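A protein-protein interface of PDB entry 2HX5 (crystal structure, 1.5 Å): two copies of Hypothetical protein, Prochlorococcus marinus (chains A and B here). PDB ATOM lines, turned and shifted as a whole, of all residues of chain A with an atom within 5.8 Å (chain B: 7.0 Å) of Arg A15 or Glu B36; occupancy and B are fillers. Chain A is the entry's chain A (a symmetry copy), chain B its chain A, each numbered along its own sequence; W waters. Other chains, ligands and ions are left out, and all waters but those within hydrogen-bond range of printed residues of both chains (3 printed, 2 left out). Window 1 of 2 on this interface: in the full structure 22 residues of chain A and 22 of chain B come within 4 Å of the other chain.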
ATOM      1  N   ARG A  12     -23.220  10.323  33.343  1.00  0.00           N
ATOM      2  CA  ARG A  12     -22.968  11.455  32.457  1.00  0.00           C
ATOM      3  C   ARG A  12     -23.130  12.780  33.174  1.00  0.00           C
ATOM      4  O   ARG A  12     -23.771  12.920  34.215  1.00  0.00           O
ATOM      5  CB  ARG A  12     -23.843  11.422  31.214  1.00  0.00           C
ATOM      6  CG  ARG A  12     -25.291  11.818  31.436  1.00  0.00           C
ATOM      7  CD  ARG A  12     -26.086  11.759  30.115  1.00  0.00           C
ATOM      8  NE  ARG A  12     -25.641  12.690  29.089  1.00  0.00           N
ATOM      9  CZ  ARG A  12     -25.376  12.394  27.785  1.00  0.00           C
ATOM     10  NH1 ARG A  12     -25.416  11.181  27.257  1.00  0.00           N
ATOM     11  NH2 ARG A  12     -25.078  13.390  26.991  1.00  0.00           N
ATOM     12  N   VAL A  13     -22.528  13.776  32.552  1.00  0.00           N
ATOM     13  CA  VAL A  13     -22.536  15.130  33.070  1.00  0.00           C
ATOM     14  C   VAL A  13     -23.377  15.987  32.111  1.00  0.00           C
ATOM     15  O   VAL A  13     -23.218  15.941  30.868  1.00  0.00           O
ATOM     16  CB  VAL A  13     -21.107  15.748  33.194  1.00  0.00           C
ATOM     17  CG1 VAL A  13     -21.168  17.120  33.831  1.00  0.00           C
ATOM     18  CG2 VAL A  13     -20.183  14.745  33.961  1.00  0.00           C
ATOM     19  N   VAL A  14     -24.303  16.734  32.710  1.00  0.00           N
ATOM     20  CA  VAL A  14     -25.194  17.641  32.002  1.00  0.00           C
ATOM     21  C   VAL A  14     -24.343  18.819  31.435  1.00  0.00           C
ATOM     22  O   VAL A  14     -23.567  19.419  32.153  1.00  0.00           O
ATOM     23  CB  VAL A  14     -26.322  18.190  32.924  1.00  0.00           C
ATOM     24  CG1 VAL A  14     -27.245  19.103  32.150  1.00  0.00           C
ATOM     25  CG2 VAL A  14     -27.093  17.015  33.604  1.00  0.00           C
ATOM     26  N   ARG A  15     -24.477  19.124  30.138  1.00  0.00           N
ATOM     27  CA  ARG A  15     -23.683  20.166  29.515  1.00  0.00           C
ATOM     28  C   ARG A  15     -24.554  21.393  29.201  1.00  0.00           C
ATOM     29  O   ARG A  15     -25.808  21.315  29.229  1.00  0.00           O
ATOM     30  CB  ARG A  15     -23.025  19.615  28.261  1.00  0.00           C
ATOM     31  CG  ARG A  15     -22.045  18.468  28.553  1.00  0.00           C
ATOM     32  CD  ARG A  15     -20.915  18.860  29.444  1.00  0.00           C
ATOM     33  NE  ARG A  15     -19.934  17.761  29.695  1.00  0.00           N
ATOM     34  CZ  ARG A  15     -19.080  17.758  30.710  1.00  0.00           C
ATOM     35  NH1 ARG A  15     -18.960  18.757  31.567  1.00  0.00           N
ATOM     36  NH2 ARG A  15     -18.263  16.742  30.850  1.00  0.00           N
ATOM     37  N   PHE A  16     -23.882  22.507  28.976  1.00  0.00           N
ATOM     38  CA  PHE A  16     -24.524  23.813  28.907  1.00  0.00           C
ATOM     39  C   PHE A  16     -25.607  23.828  27.799  1.00  0.00           C
ATOM     40  O   PHE A  16     -26.720  24.351  27.986  1.00  0.00           O
ATOM     41  CB  PHE A  16     -23.490  24.881  28.659  1.00  0.00           C
ATOM     42  CG  PHE A  16     -24.018  26.230  28.686  1.00  0.00           C
ATOM     43  CD1 PHE A  16     -24.603  26.721  29.848  1.00  0.00           C
ATOM     44  CD2 PHE A  16     -23.897  27.042  27.616  1.00  0.00           C
ATOM     45  CE1 PHE A  16     -25.086  28.003  29.872  1.00  0.00           C
ATOM     46  CE2 PHE A  16     -24.363  28.367  27.672  1.00  0.00           C
ATOM     47  CZ  PHE A  16     -24.938  28.799  28.773  1.00  0.00           C
ATOM     48  N   GLY A  17     -25.309  23.277  26.622  1.00  0.00           N
ATOM     49  CA  GLY A  17     -26.243  23.224  25.494  1.00  0.00           C
ATOM     50  C   GLY A  17     -27.462  22.361  25.720  1.00  0.00           C
ATOM     51  O   GLY A  17     -28.407  22.422  24.906  1.00  0.00           O
ATOM     52  N   ASP A  18     -27.452  21.551  26.790  1.00  0.00           N
ATOM     53  CA  ASP A  18     -28.594  20.727  27.140  1.00  0.00           C
ATOM     54  C   ASP A  18     -29.656  21.517  27.907  1.00  0.00           C
ATOM     55  O   ASP A  18     -30.746  20.939  28.186  1.00  0.00           O
ATOM     56  CB  ASP A  18     -28.168  19.573  28.024  1.00  0.00           C
ATOM     57  CG  ASP A  18     -27.139  18.663  27.370  1.00  0.00           C
ATOM     58  OD1 ASP A  18     -27.060  18.659  26.098  1.00  0.00           O
ATOM     59  OD2 ASP A  18     -26.340  18.022  28.135  1.00  0.00           O
ATOM     60  N   THR A  19     -29.381  22.754  28.290  1.00  0.00           N
ATOM     61  CA  THR A  19     -30.240  23.590  29.131  1.00  0.00           C
ATOM     62  C   THR A  19     -30.969  24.601  28.287  1.00  0.00           C
ATOM     63  O   THR A  19     -30.608  24.842  27.130  1.00  0.00           O
ATOM     64  CB  THR A  19     -29.429  24.359  30.195  1.00  0.00           C
ATOM     65  OG1 THR A  19     -28.602  25.345  29.543  1.00  0.00           O
ATOM     66  CG2 THR A  19     -28.732  23.407  31.087  1.00  0.00           C
ATOM     67  N   ARG A  32     -32.632  11.652  24.421  1.00  0.00           N
ATOM     68  CA  ARG A  32     -31.333  11.466  23.774  1.00  0.00           C
ATOM     69  C   ARG A  32     -30.337  10.770  24.715  1.00  0.00           C
ATOM     70  O   ARG A  32     -29.604   9.839  24.378  1.00  0.00           O
ATOM     71  CB  ARG A  32     -30.714  12.807  23.295  1.00  0.00           C
ATOM     72  CG  ARG A  32     -29.308  12.594  22.740  1.00  0.00           C
ATOM     73  CD  ARG A  32     -28.847  13.903  22.109  1.00  0.00           C
ATOM     74  NE  ARG A  32     -28.573  14.937  23.112  1.00  0.00           N
ATOM     75  CZ  ARG A  32     -27.455  15.059  23.808  1.00  0.00           C
ATOM     76  NH1 ARG A  32     -26.437  14.222  23.720  1.00  0.00           N
ATOM     77  NH2 ARG A  32     -27.343  16.052  24.662  1.00  0.00           N
ATOM     78  N   TRP A  33     -30.313  11.236  25.954  1.00  0.00           N
ATOM     79  CA  TRP A  33     -29.425  10.612  26.942  1.00  0.00           C
ATOM     80  C   TRP A  33     -29.748   9.131  27.151  1.00  0.00           C
ATOM     81  O   TRP A  33     -28.865   8.279  27.347  1.00  0.00           O
ATOM     82  CB  TRP A  33     -29.482  11.317  28.294  1.00  0.00           C
ATOM     83  CG  TRP A  33     -29.057  12.782  28.258  1.00  0.00           C
ATOM     84  CD1 TRP A  33     -28.494  13.463  27.240  1.00  0.00           C
ATOM     85  CD2 TRP A  33     -29.291  13.724  29.281  1.00  0.00           C
ATOM     86  NE1 TRP A  33     -28.301  14.778  27.593  1.00  0.00           N
ATOM     87  CE2 TRP A  33     -28.791  14.973  28.846  1.00  0.00           C
ATOM     88  CE3 TRP A  33     -29.865  13.628  30.554  1.00  0.00           C
ATOM     89  CZ2 TRP A  33     -28.871  16.126  29.633  1.00  0.00           C
ATOM     90  CZ3 TRP A  33     -29.917  14.759  31.325  1.00  0.00           C
ATOM     91  CH2 TRP A  33     -29.422  15.993  30.865  1.00  0.00           C
ATOM     92  N   THR A  82     -26.993  22.344  34.508  1.00  0.00           N
ATOM     93  CA  THR A  82     -25.697  22.235  33.849  1.00  0.00           C
ATOM     94  C   THR A  82     -24.593  21.871  34.870  1.00  0.00           C
ATOM     95  O   THR A  82     -24.476  22.471  35.953  1.00  0.00           O
ATOM     96  CB  THR A  82     -25.349  23.489  32.933  1.00  0.00           C
ATOM     97  OG1 THR A  82     -23.934  23.672  32.856  1.00  0.00           O
ATOM     98  CG2 THR A  82     -25.949  24.770  33.463  1.00  0.00           C
ATOM     99  N   GLY A  83     -23.790  20.883  34.515  1.00  0.00           N
ATOM    100  CA  GLY A  83     -22.718  20.420  35.343  1.00  0.00           C
ATOM    101  C   GLY A  83     -23.133  19.348  36.329  1.00  0.00           C
ATOM    102  O   GLY A  83     -22.242  18.815  36.976  1.00  0.00           O
ATOM    103  N   LEU B  10      -9.062  14.344  24.632  1.00  0.00           N
ATOM    104  CA  LEU B  10     -10.311  13.835  25.110  1.00  0.00           C
ATOM    105  C   LEU B  10     -10.810  12.812  24.098  1.00  0.00           C
ATOM    106  O   LEU B  10     -10.208  12.615  23.036  1.00  0.00           O
ATOM    107  CB  LEU B  10     -11.304  14.997  25.333  1.00  0.00           C
ATOM    108  CG  LEU B  10     -10.812  16.073  26.340  1.00  0.00           C
ATOM    109  CD1 LEU B  10     -11.679  17.324  26.316  1.00  0.00           C
ATOM    110  CD2 LEU B  10     -10.711  15.486  27.777  1.00  0.00           C
ATOM    111  N   ARG B  12     -14.460  10.719  22.467  1.00  0.00           N
ATOM    112  CA  ARG B  12     -15.886  10.414  22.437  1.00  0.00           C
ATOM    113  C   ARG B  12     -16.233   9.447  21.323  1.00  0.00           C
ATOM    114  O   ARG B  12     -15.523   9.258  20.336  1.00  0.00           O
ATOM    115  CB  ARG B  12     -16.743  11.665  22.329  1.00  0.00           C
ATOM    116  CG  ARG B  12     -16.772  12.309  20.955  1.00  0.00           C
ATOM    117  CD  ARG B  12     -17.674  13.561  20.953  1.00  0.00           C
ATOM    118  NE  ARG B  12     -19.080  13.306  21.230  1.00  0.00           N
ATOM    119  CZ  ARG B  12     -19.861  13.965  22.131  1.00  0.00           C
ATOM    120  NH1 ARG B  12     -19.440  14.910  22.957  1.00  0.00           N
ATOM    121  NH2 ARG B  12     -21.131  13.652  22.167  1.00  0.00           N
ATOM    122  N   LEU B  30     -20.905  18.389  15.033  1.00  0.00           N
ATOM    123  CA  LEU B  30     -19.481  18.619  15.362  1.00  0.00           C
ATOM    124  C   LEU B  30     -19.319  19.764  16.354  1.00  0.00           C
ATOM    125  O   LEU B  30     -18.472  19.723  17.216  1.00  0.00           O
ATOM    126  CB  LEU B  30     -18.636  18.908  14.120  1.00  0.00           C
ATOM    127  CG  LEU B  30     -17.121  18.671  14.314  1.00  0.00           C
ATOM    128  CD1 LEU B  30     -16.760  17.220  14.218  1.00  0.00           C
ATOM    129  CD2 LEU B  30     -16.288  19.526  13.285  1.00  0.00           C
ATOM    130  N   PHE B  31     -20.097  20.817  16.149  1.00  0.00           N
ATOM    131  CA  PHE B  31     -19.975  21.993  17.029  1.00  0.00           C
ATOM    132  C   PHE B  31     -20.428  21.748  18.422  1.00  0.00           C
ATOM    133  O   PHE B  31     -19.866  22.270  19.386  1.00  0.00           O
ATOM    134  CB  PHE B  31     -20.736  23.164  16.388  1.00  0.00           C
ATOM    135  CG  PHE B  31     -20.114  23.694  15.131  1.00  0.00           C
ATOM    136  CD1 PHE B  31     -18.902  24.386  15.170  1.00  0.00           C
ATOM    137  CD2 PHE B  31     -20.735  23.489  13.931  1.00  0.00           C
ATOM    138  CE1 PHE B  31     -18.319  24.847  14.029  1.00  0.00           C
ATOM    139  CE2 PHE B  31     -20.146  23.943  12.769  1.00  0.00           C
ATOM    140  CZ  PHE B  31     -18.946  24.658  12.840  1.00  0.00           C
ATOM    141  N   ARG B  32     -21.504  20.968  18.555  1.00  0.00           N
ATOM    142  CA  ARG B  32     -21.924  20.534  19.888  1.00  0.00           C
ATOM    143  C   ARG B  32     -20.809  19.746  20.593  1.00  0.00           C
ATOM    144  O   ARG B  32     -20.472  19.924  21.765  1.00  0.00           O
ATOM    145  CB  ARG B  32     -23.207  19.660  19.850  1.00  0.00           C
ATOM    146  CG  ARG B  32     -23.545  19.122  21.238  1.00  0.00           C
ATOM    147  CD  ARG B  32     -24.911  18.449  21.163  1.00  0.00           C
ATOM    148  NE  ARG B  32     -24.872  17.196  20.403  1.00  0.00           N
ATOM    149  CZ  ARG B  32     -24.492  16.020  20.876  1.00  0.00           C
ATOM    150  NH1 ARG B  32     -24.048  15.828  22.105  1.00  0.00           N
ATOM    151  NH2 ARG B  32     -24.529  14.974  20.081  1.00  0.00           N
ATOM    152  N   TRP B  33     -20.203  18.837  19.846  1.00  0.00           N
ATOM    153  CA  TRP B  33     -19.097  18.057  20.413  1.00  0.00           C
ATOM    154  C   TRP B  33     -17.935  18.948  20.858  1.00  0.00           C
ATOM    155  O   TRP B  33     -17.263  18.706  21.875  1.00  0.00           O
ATOM    156  CB  TRP B  33     -18.563  17.017  19.433  1.00  0.00           C
ATOM    157  CG  TRP B  33     -19.591  15.975  18.999  1.00  0.00           C
ATOM    158  CD1 TRP B  33     -20.828  15.769  19.491  1.00  0.00           C
ATOM    159  CD2 TRP B  33     -19.450  15.100  17.903  1.00  0.00           C
ATOM    160  NE1 TRP B  33     -21.456  14.760  18.799  1.00  0.00           N
ATOM    161  CE2 TRP B  33     -20.633  14.331  17.806  1.00  0.00           C
ATOM    162  CE3 TRP B  33     -18.414  14.870  16.990  1.00  0.00           C
ATOM    163  CZ2 TRP B  33     -20.817  13.364  16.813  1.00  0.00           C
ATOM    164  CZ3 TRP B  33     -18.596  13.905  16.036  1.00  0.00           C
ATOM    165  CH2 TRP B  33     -19.787  13.160  15.954  1.00  0.00           C
ATOM    166  N   CYS B  34     -17.642  19.968  20.053  1.00  0.00           N
ATOM    167  CA  CYS B  34     -16.597  20.918  20.449  1.00  0.00           C
ATOM    168  C   CYS B  34     -16.913  21.627  21.743  1.00  0.00           C
ATOM    169  O   CYS B  34     -16.131  21.643  22.692  1.00  0.00           O
ATOM    170  CB  CYS B  34     -16.410  21.952  19.362  1.00  0.00           C
ATOM    171  SG  CYS B  34     -15.654  21.401  17.800  1.00  0.00           S
ATOM    172  N   HIS B  35     -18.122  22.162  21.829  1.00  0.00           N
ATOM    173  CA  HIS B  35     -18.506  22.896  23.012  1.00  0.00           C
ATOM    174  C   HIS B  35     -18.476  21.996  24.236  1.00  0.00           C
ATOM    175  O   HIS B  35     -17.955  22.343  25.313  1.00  0.00           O
ATOM    176  CB  HIS B  35     -19.858  23.562  22.827  1.00  0.00           C
ATOM    177  CG  HIS B  35     -20.216  24.612  23.850  1.00  0.00           C
ATOM    178  ND1 HIS B  35     -20.470  24.336  25.184  1.00  0.00           N
ATOM    179  CD2 HIS B  35     -20.415  25.941  23.690  1.00  0.00           C
ATOM    180  CE1 HIS B  35     -20.827  25.472  25.780  1.00  0.00           C
ATOM    181  NE2 HIS B  35     -20.755  26.456  24.910  1.00  0.00           N
ATOM    182  N   GLU B  36     -19.035  20.791  24.077  1.00  0.00           N
ATOM    183  CA  GLU B  36     -19.003  19.858  25.212  1.00  0.00           C
ATOM    184  C   GLU B  36     -17.585  19.468  25.605  1.00  0.00           C
ATOM    185  O   GLU B  36     -17.291  19.311  26.784  1.00  0.00           O
ATOM    186  CB  GLU B  36     -19.769  18.580  24.884  1.00  0.00           C
ATOM    187  CG  GLU B  36     -21.251  18.759  24.679  1.00  0.00           C
ATOM    188  CD  GLU B  36     -22.072  17.487  24.487  1.00  0.00           C
ATOM    189  OE1 GLU B  36     -21.448  16.411  24.509  1.00  0.00           O
ATOM    190  OE2 GLU B  36     -23.308  17.605  24.358  1.00  0.00           O
ATOM    191  N   SER B  37     -16.678  19.310  24.640  1.00  0.00           N
ATOM    192  CA  SER B  37     -15.281  18.988  24.990  1.00  0.00           C
ATOM    193  C   SER B  37     -14.564  20.131  25.682  1.00  0.00           C
ATOM    194  O   SER B  37     -13.677  19.915  26.496  1.00  0.00           O
ATOM    195  CB  SER B  37     -14.479  18.512  23.778  1.00  0.00           C
ATOM    196  OG  SER B  37     -14.074  19.584  22.935  1.00  0.00           O
ATOM    197  N   TRP B  38     -14.930  21.362  25.333  1.00  0.00           N
ATOM    198  CA  TRP B  38     -14.402  22.541  26.006  1.00  0.00           C
ATOM    199  C   TRP B  38     -14.860  22.531  27.489  1.00  0.00           C
ATOM    200  O   TRP B  38     -14.066  22.702  28.413  1.00  0.00           O
ATOM    201  CB  TRP B  38     -14.856  23.803  25.289  1.00  0.00           C
ATOM    202  CG  TRP B  38     -14.579  25.076  26.057  1.00  0.00           C
ATOM    203  CD1 TRP B  38     -13.386  25.506  26.501  1.00  0.00           C
ATOM    204  CD2 TRP B  38     -15.537  26.069  26.417  1.00  0.00           C
ATOM    205  NE1 TRP B  38     -13.518  26.732  27.120  1.00  0.00           N
ATOM    206  CE2 TRP B  38     -14.840  27.101  27.089  1.00  0.00           C
ATOM    207  CE3 TRP B  38     -16.916  26.199  26.228  1.00  0.00           C
ATOM    208  CZ2 TRP B  38     -15.507  28.247  27.630  1.00  0.00           C
ATOM    209  CZ3 TRP B  38     -17.541  27.338  26.688  1.00  0.00           C
ATOM    210  CH2 TRP B  38     -16.844  28.335  27.398  1.00  0.00           C
ATOM    211  N   GLU B  39     -16.156  22.275  27.708  1.00  0.00           N
ATOM    212  CA  GLU B  39     -16.656  22.148  29.081  1.00  0.00           C
ATOM    213  C   GLU B  39     -15.914  21.031  29.815  1.00  0.00           C
ATOM    214  O   GLU B  39     -15.540  21.174  30.977  1.00  0.00           O
ATOM    215  CB  GLU B  39     -18.165  21.862  29.062  1.00  0.00           C
ATOM    216  CG  GLU B  39     -18.993  22.963  28.447  1.00  0.00           C
ATOM    217  CD  GLU B  39     -20.453  22.565  28.271  1.00  0.00           C
ATOM    218  OE1 GLU B  39     -21.160  22.445  29.310  1.00  0.00           O
ATOM    219  OE2 GLU B  39     -20.841  22.376  27.094  1.00  0.00           O
ATOM    220  N   GLU B  40     -15.758  19.871  29.167  1.00  0.00           N
ATOM    221  CA  GLU B  40     -15.014  18.727  29.747  1.00  0.00           C
ATOM    222  C   GLU B  40     -13.584  19.085  30.098  1.00  0.00           C
ATOM    223  O   GLU B  40     -13.055  18.674  31.152  1.00  0.00           O
ATOM    224  CB  GLU B  40     -15.010  17.512  28.811  1.00  0.00           C
ATOM    225  CG  GLU B  40     -14.514  16.290  29.480  1.00  0.00           C
ATOM    226  CD  GLU B  40     -14.515  15.068  28.570  1.00  0.00           C
ATOM    227  OE1 GLU B  40     -15.010  15.147  27.429  1.00  0.00           O
ATOM    228  OE2 GLU B  40     -13.965  14.017  28.999  1.00  0.00           O
ATOM    229  N   SER B  41     -12.955  19.862  29.228  1.00  0.00           N
ATOM    230  CA  SER B  41     -11.596  20.314  29.492  1.00  0.00           C
ATOM    231  C   SER B  41     -11.447  21.201  30.718  1.00  0.00           C
ATOM    232  O   SER B  41     -10.586  21.020  31.543  1.00  0.00           O
ATOM    233  CB  SER B  41     -11.080  21.032  28.249  1.00  0.00           C
ATOM    234  OG  SER B  41      -9.699  21.382  28.410  1.00  0.00           O
ATOM    235  N   LEU B  42     -12.390  22.129  30.849  1.00  0.00           N
ATOM    236  CA  LEU B  42     -12.377  23.010  31.985  1.00  0.00           C
ATOM    237  C   LEU B  42     -12.573  22.199  33.270  1.00  0.00           C
ATOM    238  O   LEU B  42     -11.859  22.429  34.253  1.00  0.00           O
ATOM    239  CB  LEU B  42     -13.479  24.066  31.874  1.00  0.00           C
ATOM    240  CG  LEU B  42     -13.392  25.046  30.675  1.00  0.00           C
ATOM    241  CD1 LEU B  42     -14.662  25.943  30.701  1.00  0.00           C
ATOM    242  CD2 LEU B  42     -12.100  25.841  30.709  1.00  0.00           C
ATOM    243  N   GLU B  43     -13.516  21.252  33.232  1.00  0.00           N
ATOM    244  CA  GLU B  43     -13.797  20.332  34.365  1.00  0.00           C
ATOM    245  C   GLU B  43     -12.546  19.510  34.763  1.00  0.00           C
ATOM    246  O   GLU B  43     -12.176  19.409  35.930  1.00  0.00           O
ATOM    247  CB  GLU B  43     -14.933  19.425  33.909  1.00  0.00           C
ATOM    248  CG  GLU B  43     -15.466  18.329  34.778  1.00  0.00           C
ATOM    249  CD  GLU B  43     -16.634  17.678  34.004  1.00  0.00           C
ATOM    250  OE1 GLU B  43     -16.402  16.740  33.183  1.00  0.00           O
ATOM    251  OE2 GLU B  43     -17.744  18.250  34.138  1.00  0.00           O
ATOM    252  N   PRO B  49     -18.117  24.235  37.385  1.00  0.00           N
ATOM    253  CA  PRO B  49     -19.132  24.780  36.465  1.00  0.00           C
ATOM    254  C   PRO B  49     -19.887  25.972  37.034  1.00  0.00           C
ATOM    255  O   PRO B  49     -20.239  26.880  36.278  1.00  0.00           O
ATOM    256  CB  PRO B  49     -20.153  23.609  36.287  1.00  0.00           C
ATOM    257  CG  PRO B  49     -19.785  22.570  37.265  1.00  0.00           C
ATOM    258  CD  PRO B  49     -18.291  22.771  37.534  1.00  0.00           C
ATOM    259  N   MET B  88     -10.030  13.582  20.369  1.00  0.00           N
ATOM    260  CA  MET B  88     -10.183  15.021  20.239  1.00  0.00           C
ATOM    261  C   MET B  88      -9.005  15.722  20.879  1.00  0.00           C
ATOM    262  O   MET B  88      -8.662  15.448  22.006  1.00  0.00           O
ATOM    263  CB  MET B  88     -11.444  15.471  20.924  1.00  0.00           C
ATOM    264  CG  MET B  88     -12.724  14.872  20.260  1.00  0.00           C
ATOM    265  SD  MET B  88     -14.348  15.493  21.068  1.00  0.00           S
ATOM    266  CE  MET B  88     -14.222  14.492  22.776  1.00  0.00           C
ATOM    267  N   PHE B 104     -10.084  22.552  17.637  1.00  0.00           N
ATOM    268  CA  PHE B 104     -10.448  21.204  17.948  1.00  0.00           C
ATOM    269  C   PHE B 104     -10.066  20.354  16.765  1.00  0.00           C
ATOM    270  O   PHE B 104     -10.522  20.608  15.634  1.00  0.00           O
ATOM    271  CB  PHE B 104     -11.964  21.117  18.137  1.00  0.00           C
ATOM    272  CG  PHE B 104     -12.521  22.031  19.210  1.00  0.00           C
ATOM    273  CD1 PHE B 104     -12.840  23.347  18.962  1.00  0.00           C
ATOM    274  CD2 PHE B 104     -12.708  21.535  20.503  1.00  0.00           C
ATOM    275  CE1 PHE B 104     -13.354  24.171  19.945  1.00  0.00           C
ATOM    276  CE2 PHE B 104     -13.228  22.350  21.459  1.00  0.00           C
ATOM    277  CZ  PHE B 104     -13.559  23.671  21.178  1.00  0.00           C
HETATM  278  O   HOH W   1     -24.858  16.384  26.206  1.00  0.00           O
HETATM  279  O   HOH W   2     -24.615  19.814  24.874  1.00  0.00           O
HETATM  280  O   HOH W   3     -23.007  22.009  25.501  1.00  0.00           O
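Among the printed residues, merely in contact across the chains: Val A13 with Glu B43, Arg A15 with Glu B36, Arg A15 with Glu B39, Arg A15 with Glu B40 and Phe A16 with His B35.
Hydrophobic or aromatic side chains of chain A that line the printed part of chain B: Val A13 and Phe A16.
Among the printed residues, 8 pairs touch across the chains.
Arg B32 touches its own counterpart, Arg A32.
3 positions are printed for both chains.
Water W2 bridges the side-chain carboxylate of Glu B36 (2.6 Å) and the side-chain carboxylate of Asp A18 (3.0 Å).
Water W1 lies within hydrogen-bond range of the side-chain carboxylate (OE2) of Glu B36, the side-chain carboxylate (OD2) of Asp A18, the guanidinium group (NH2) of Arg A32 and the guanidinium group (NH2) of Arg A12.
Water W3 lies within hydrogen-bond range of OE2 of Glu B39 (2.7 Å), N of Gly A17 (2.9 Å) and ND1 of His B35 (3.5 Å).
ND1 of His B35 lies within hydrogen-bond range of OE2 of Glu B39 (2.8 Å).
OG1 of Thr A19 sits at hydrogen-bond distance from O of Phe A16, 2.6 Å away.
NH1 of Arg B32 is in salt-bridge range of OE2 of Glu B36.
The backbone NH (N) of Arg A15 is in hydrogen-bond range of the side-chain carboxylate (OD2) of Asp A18, at 2.9 Å.
NH2 of Arg A32 lies within salt-bridge range of OD1 of Asp A18 (3.0 Å).
OE1 of Glu B36 is in salt-bridge range of NH1 of Arg B12, at 2.9 Å.
The guanidinium group of Arg A15 is in salt-bridge range of the side-chain carboxylate of Glu B43, at 2.9 Å.
OE1 of Glu B39 lies within hydrogen-bond range of N of Phe A16, 2.7 Å away.
NH1 of Arg B32 sits close to NH1 of Arg A32 (3.3 Å).
Arg A15 touches just these residues of chain B: Glu B36 (3.97 Å), Glu B39 (3.4 Å), Glu B40 (3.9 Å) and Glu B43 (2.9 Å).
Printed residues of chain B within 4 Å of Phe A16: His B35 and Glu B39.
Printed residues of chain B within 4 Å of Arg A32: Arg B32 (3.3 Å).
Glu B36 touches one residue of chain A.
Of the printed residues of chain A, Glu B39 touches Arg A15 and Phe A16.
The nearest residue of chain B that does not touch Arg A15 is His B35 (6.2 Å).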
